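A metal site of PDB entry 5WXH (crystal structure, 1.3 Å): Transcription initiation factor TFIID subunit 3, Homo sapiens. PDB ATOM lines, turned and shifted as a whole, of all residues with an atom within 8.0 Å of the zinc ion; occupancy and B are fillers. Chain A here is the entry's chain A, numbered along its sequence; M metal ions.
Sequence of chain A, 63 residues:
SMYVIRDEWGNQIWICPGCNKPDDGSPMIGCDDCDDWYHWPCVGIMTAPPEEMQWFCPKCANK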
ATOM      1  N   PRO A  17      -0.559 -14.228 -12.270  1.00  0.00           N
ATOM      2  CA  PRO A  17      -0.277 -15.551 -12.843  1.00  0.00           C
ATOM      3  C   PRO A  17       1.207 -15.866 -12.939  1.00  0.00           C
ATOM      4  O   PRO A  17       1.562 -17.051 -13.090  1.00  0.00           O
ATOM      5  CB  PRO A  17      -0.926 -15.478 -14.236  1.00  0.00           C
ATOM      6  CG  PRO A  17      -1.953 -14.389 -14.113  1.00  0.00           C
ATOM      7  CD  PRO A  17      -1.355 -13.391 -13.180  1.00  0.00           C
ATOM      8  N   GLY A  30      -2.238  -4.607 -16.245  1.00  0.00           N
ATOM      9  CA  GLY A  30      -3.365  -5.414 -16.659  1.00  0.00           C
ATOM     10  C   GLY A  30      -3.301  -5.746 -18.147  1.00  0.00           C
ATOM     11  O   GLY A  30      -3.030  -4.877 -18.971  1.00  0.00           O
ATOM     12  N   CYS A  31      -3.570  -7.004 -18.468  1.00  0.00           N
ATOM     13  CA  CYS A  31      -3.498  -7.444 -19.857  1.00  0.00           C
ATOM     14  C   CYS A  31      -4.713  -6.940 -20.625  1.00  0.00           C
ATOM     15  O   CYS A  31      -5.853  -7.178 -20.218  1.00  0.00           O
ATOM     16  CB  CYS A  31      -3.459  -8.966 -19.925  1.00  0.00           C
ATOM     17  SG  CYS A  31      -3.377  -9.571 -21.651  1.00  0.00           S
ATOM     18  N   ASP A  32      -4.466  -6.282 -21.762  1.00  0.00           N
ATOM     19  CA  ASP A  32      -5.543  -5.721 -22.560  1.00  0.00           C
ATOM     20  C   ASP A  32      -6.241  -6.753 -23.428  1.00  0.00           C
ATOM     21  O   ASP A  32      -7.153  -6.397 -24.187  1.00  0.00           O
ATOM     22  CB  ASP A  32      -5.032  -4.514 -23.353  1.00  0.00           C
ATOM     23  CG  ASP A  32      -4.695  -3.342 -22.447  1.00  0.00           C
ATOM     24  OD1 ASP A  32      -5.476  -3.107 -21.509  1.00  0.00           O
ATOM     25  OD2 ASP A  32      -3.655  -2.675 -22.650  1.00  0.00           O
ATOM     26  N   ASP A  33      -5.848  -8.016 -23.333  1.00  0.00           N
ATOM     27  CA  ASP A  33      -6.558  -9.110 -23.988  1.00  0.00           C
ATOM     28  C   ASP A  33      -7.382  -9.865 -22.946  1.00  0.00           C
ATOM     29  O   ASP A  33      -8.613  -9.788 -22.952  1.00  0.00           O
ATOM     30  CB  ASP A  33      -5.558 -10.029 -24.696  1.00  0.00           C
ATOM     31  CG  ASP A  33      -6.225 -11.143 -25.505  1.00  0.00           C
ATOM     32  OD1 ASP A  33      -7.359 -11.555 -25.200  1.00  0.00           O
ATOM     33  OD2 ASP A  33      -5.565 -11.605 -26.458  1.00  0.00           O
ATOM     34  N   CYS A  34      -6.712 -10.574 -22.023  1.00  0.00           N
ATOM     35  CA  CYS A  34      -7.378 -11.476 -21.085  1.00  0.00           C
ATOM     36  C   CYS A  34      -7.777 -10.827 -19.757  1.00  0.00           C
ATOM     37  O   CYS A  34      -8.508 -11.452 -18.985  1.00  0.00           O
ATOM     38  CB  CYS A  34      -6.513 -12.701 -20.803  1.00  0.00           C
ATOM     39  SG  CYS A  34      -5.081 -12.359 -19.777  1.00  0.00           S
ATOM     40  N   ASP A  35      -7.284  -9.627 -19.444  1.00  0.00           N
ATOM     41  CA  ASP A  35      -7.640  -8.871 -18.245  1.00  0.00           C
ATOM     42  C   ASP A  35      -7.015  -9.418 -16.957  1.00  0.00           C
ATOM     43  O   ASP A  35      -7.394  -8.969 -15.873  1.00  0.00           O
ATOM     44  CB  ASP A  35      -9.154  -8.688 -18.085  1.00  0.00           C
ATOM     45  CG  ASP A  35      -9.514  -7.517 -17.204  1.00  0.00           C
ATOM     46  OD1 ASP A  35      -8.800  -6.493 -17.247  1.00  0.00           O
ATOM     47  OD2 ASP A  35     -10.528  -7.612 -16.471  1.00  0.00           O
ATOM     48  N   ASP A  36      -6.086 -10.368 -17.037  1.00  0.00           N
ATOM     49  CA  ASP A  36      -5.333 -10.744 -15.837  1.00  0.00           C
ATOM     50  C   ASP A  36      -4.387  -9.599 -15.435  1.00  0.00           C
ATOM     51  O   ASP A  36      -3.976  -8.788 -16.262  1.00  0.00           O
ATOM     52  CB  ASP A  36      -4.505 -12.016 -16.075  1.00  0.00           C
ATOM     53  CG  ASP A  36      -5.348 -13.270 -16.157  1.00  0.00           C
ATOM     54  OD1 ASP A  36      -6.503 -13.256 -15.700  1.00  0.00           O
ATOM     55  OD2 ASP A  36      -4.834 -14.293 -16.670  1.00  0.00           O
ATOM     56  N   TRP A  37      -4.043  -9.570 -14.157  1.00  0.00           N
ATOM     57  CA  TRP A  37      -3.154  -8.547 -13.603  1.00  0.00           C
ATOM     58  C   TRP A  37      -1.861  -9.198 -13.122  1.00  0.00           C
ATOM     59  O   TRP A  37      -1.900 -10.221 -12.427  1.00  0.00           O
ATOM     60  CB  TRP A  37      -3.835  -7.808 -12.449  1.00  0.00           C
ATOM     61  CG  TRP A  37      -4.863  -6.828 -12.934  1.00  0.00           C
ATOM     62  CD1 TRP A  37      -6.172  -7.079 -13.247  1.00  0.00           C
ATOM     63  CD2 TRP A  37      -4.658  -5.427 -13.196  1.00  0.00           C
ATOM     64  NE1 TRP A  37      -6.791  -5.926 -13.673  1.00  0.00           N
ATOM     65  CE2 TRP A  37      -5.880  -4.901 -13.644  1.00  0.00           C
ATOM     66  CE3 TRP A  37      -3.558  -4.578 -13.066  1.00  0.00           C
ATOM     67  CZ2 TRP A  37      -6.035  -3.555 -13.978  1.00  0.00           C
ATOM     68  CZ3 TRP A  37      -3.717  -3.246 -13.399  1.00  0.00           C
ATOM     69  CH2 TRP A  37      -4.936  -2.756 -13.840  1.00  0.00           C
ATOM     70  N   TYR A  38      -0.731  -8.601 -13.484  1.00  0.00           N
ATOM     71  CA  TYR A  38       0.593  -9.121 -13.145  1.00  0.00           C
ATOM     72  C   TYR A  38       1.379  -8.071 -12.373  1.00  0.00           C
ATOM     73  O   TYR A  38       1.292  -6.880 -12.688  1.00  0.00           O
ATOM     74  CB  TYR A  38       1.381  -9.445 -14.409  1.00  0.00           C
ATOM     75  CG  TYR A  38       0.954 -10.681 -15.170  1.00  0.00           C
ATOM     76  CD1 TYR A  38       1.732 -11.830 -15.145  1.00  0.00           C
ATOM     77  CD2 TYR A  38      -0.210 -10.694 -15.927  1.00  0.00           C
ATOM     78  CE1 TYR A  38       1.360 -12.958 -15.862  1.00  0.00           C
ATOM     79  CE2 TYR A  38      -0.588 -11.827 -16.639  1.00  0.00           C
ATOM     80  CZ  TYR A  38       0.205 -12.942 -16.599  1.00  0.00           C
ATOM     81  OH  TYR A  38      -0.170 -14.067 -17.299  1.00  0.00           O
ATOM     82  N   TRP A  55      -0.799  -3.195 -23.310  1.00  0.00           N
ATOM     83  CA  TRP A  55       0.101  -4.229 -22.817  1.00  0.00           C
ATOM     84  C   TRP A  55      -0.601  -5.573 -22.856  1.00  0.00           C
ATOM     85  O   TRP A  55      -1.773  -5.696 -22.476  1.00  0.00           O
ATOM     86  CB  TRP A  55       0.604  -3.931 -21.396  1.00  0.00           C
ATOM     87  CG  TRP A  55       1.504  -5.016 -20.895  1.00  0.00           C
ATOM     88  CD1 TRP A  55       2.824  -5.177 -21.178  1.00  0.00           C
ATOM     89  CD2 TRP A  55       1.145  -6.116 -20.048  1.00  0.00           C
ATOM     90  NE1 TRP A  55       3.322  -6.300 -20.557  1.00  0.00           N
ATOM     91  CE2 TRP A  55       2.303  -6.888 -19.844  1.00  0.00           C
ATOM     92  CE3 TRP A  55      -0.045  -6.509 -19.434  1.00  0.00           C
ATOM     93  CZ2 TRP A  55       2.307  -8.044 -19.067  1.00  0.00           C
ATOM     94  CZ3 TRP A  55      -0.042  -7.649 -18.642  1.00  0.00           C
ATOM     95  CH2 TRP A  55       1.131  -8.399 -18.474  1.00  0.00           C
ATOM     96  N   PHE A  56       0.116  -6.586 -23.339  1.00  0.00           N
ATOM     97  CA  PHE A  56      -0.389  -7.940 -23.411  1.00  0.00           C
ATOM     98  C   PHE A  56       0.524  -8.889 -22.647  1.00  0.00           C
ATOM     99  O   PHE A  56       1.746  -8.775 -22.718  1.00  0.00           O
ATOM    100  CB  PHE A  56      -0.527  -8.365 -24.873  1.00  0.00           C
ATOM    101  CG  PHE A  56      -1.449  -7.473 -25.648  1.00  0.00           C
ATOM    102  CD1 PHE A  56      -2.828  -7.596 -25.487  1.00  0.00           C
ATOM    103  CD2 PHE A  56      -0.954  -6.495 -26.489  1.00  0.00           C
ATOM    104  CE1 PHE A  56      -3.691  -6.754 -26.173  1.00  0.00           C
ATOM    105  CE2 PHE A  56      -1.813  -5.655 -27.192  1.00  0.00           C
ATOM    106  CZ  PHE A  56      -3.178  -5.796 -27.031  1.00  0.00           C
ATOM    107  N   CYS A  57      -0.091  -9.801 -21.882  1.00  0.00           N
ATOM    108  CA  CYS A  57       0.657 -10.698 -21.017  1.00  0.00           C
ATOM    109  C   CYS A  57       1.363 -11.746 -21.858  1.00  0.00           C
ATOM    110  O   CYS A  57       1.067 -11.888 -23.044  1.00  0.00           O
ATOM    111  CB  CYS A  57      -0.285 -11.330 -19.994  1.00  0.00           C
ATOM    112  SG  CYS A  57      -1.298 -12.667 -20.633  1.00  0.00           S
ATOM    113  N   PRO A  58       2.304 -12.510 -21.281  1.00  0.00           N
ATOM    114  CA  PRO A  58       3.025 -13.509 -22.091  1.00  0.00           C
ATOM    115  C   PRO A  58       2.119 -14.524 -22.759  1.00  0.00           C
ATOM    116  O   PRO A  58       2.381 -14.922 -23.910  1.00  0.00           O
ATOM    117  CB  PRO A  58       3.979 -14.163 -21.084  1.00  0.00           C
ATOM    118  CG  PRO A  58       4.196 -13.115 -20.053  1.00  0.00           C
ATOM    119  CD  PRO A  58       2.900 -12.362 -19.938  1.00  0.00           C
ATOM    120  N   LYS A  59       1.066 -14.960 -22.080  1.00  0.00           N
ATOM    121  CA  LYS A  59       0.132 -15.916 -22.669  1.00  0.00           C
ATOM    122  C   LYS A  59      -0.534 -15.338 -23.906  1.00  0.00           C
ATOM    123  O   LYS A  59      -0.605 -16.006 -24.954  1.00  0.00           O
ATOM    124  CB  LYS A  59      -0.920 -16.312 -21.623  1.00  0.00           C
ATOM    125  CG  LYS A  59      -1.944 -17.323 -22.116  1.00  0.00           C
ATOM    126  CD  LYS A  59      -2.968 -17.642 -21.034  1.00  0.00           C
ATOM    127  CE  LYS A  59      -3.798 -16.415 -20.669  1.00  0.00           C
ATOM    128  NZ  LYS A  59      -4.565 -15.898 -21.830  1.00  0.00           N
ATOM    129  N   CYS A  60      -1.022 -14.097 -23.822  1.00  0.00           N
ATOM    130  CA  CYS A  60      -1.785 -13.509 -24.927  1.00  0.00           C
ATOM    131  C   CYS A  60      -0.882 -13.002 -26.047  1.00  0.00           C
ATOM    132  O   CYS A  60      -1.295 -13.024 -27.216  1.00  0.00           O
ATOM    133  CB  CYS A  60      -2.649 -12.360 -24.413  1.00  0.00           C
ATOM    134  SG  CYS A  60      -3.941 -12.910 -23.315  1.00  0.00           S
ATOM    135  N   ALA A  61       0.323 -12.533 -25.718  1.00  0.00           N
ATOM    136  CA  ALA A  61       1.191 -11.938 -26.723  1.00  0.00           C
ATOM    137  C   ALA A  61       1.474 -12.898 -27.869  1.00  0.00           C
ATOM    138  O   ALA A  61       1.716 -12.466 -28.998  1.00  0.00           O
ATOM    139  CB  ALA A  61       2.507 -11.500 -26.085  1.00  0.00           C
ATOM    140  N   LYS A  63      -0.730 -15.124 -29.008  1.00  0.00           N
ATOM    141  CA  LYS A  63      -1.983 -15.539 -29.617  1.00  0.00           C
ATOM    142  C   LYS A  63      -2.413 -14.590 -30.739  1.00  0.00           C
ATOM    143  O   LYS A  63      -3.614 -14.366 -30.950  1.00  0.00           O
ATOM    144  CB  LYS A  63      -3.091 -15.626 -28.559  1.00  0.00           C
ATOM    145  CG  LYS A  63      -2.872 -16.714 -27.525  1.00  0.00           C
ATOM    146  CD  LYS A  63      -4.001 -16.712 -26.505  1.00  0.00           C
ATOM    147  CE  LYS A  63      -3.770 -17.768 -25.425  1.00  0.00           C
ATOM    148  NZ  LYS A  63      -4.798 -17.713 -24.354  1.00  0.00           N
ATOM    149  OXT LYS A  63      -1.581 -14.029 -31.458  1.00  0.00           O
HETATM  150 ZN    ZN M   1      -3.408 -11.886 -21.287  1.00  0.00          ZN
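The side-chain sulfur (SG) of Cys 34 lies close to the backbone NH (N) of Asp 36, 3.5 Å away. The side-chain sulfur (SG) of Cys 60 lies close to the side-chain amino group (NZ) of Lys 59 (3.4 Å). SG of Cys 60 lies close to OD2 of Asp 33, 3.8 Å away. SG of Cys 57 sits close to N of Lys 59. The side-chain hydroxyl (OH) of Tyr 38 lies close to the side-chain sulfur (SG) of Cys 57 (3.8 Å). SG of Cys 31 lies close to N of Asp 33, 3.4 Å away. N of Cys 31 lies within hydrogen-bond range of O of Asp 36 (2.9 Å).
Of the 18 residues printed, 4 come within 4 Å of the zinc ion. The nearest printed residue that does not touch the zinc ion is Lys 59 (4.2 Å).
The zinc ion is bound by the side-chain sulfur (SG) of Cys 34 (2.3 Å), the side-chain sulfur (SG) of Cys 60 (2.3 Å), the side-chain sulfur (SG) of Cys 57 (2.3 Å) and the side-chain sulfur (SG) of Cys 31 (2.3 Å). The zinc ion has four donor atoms within binding distance.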
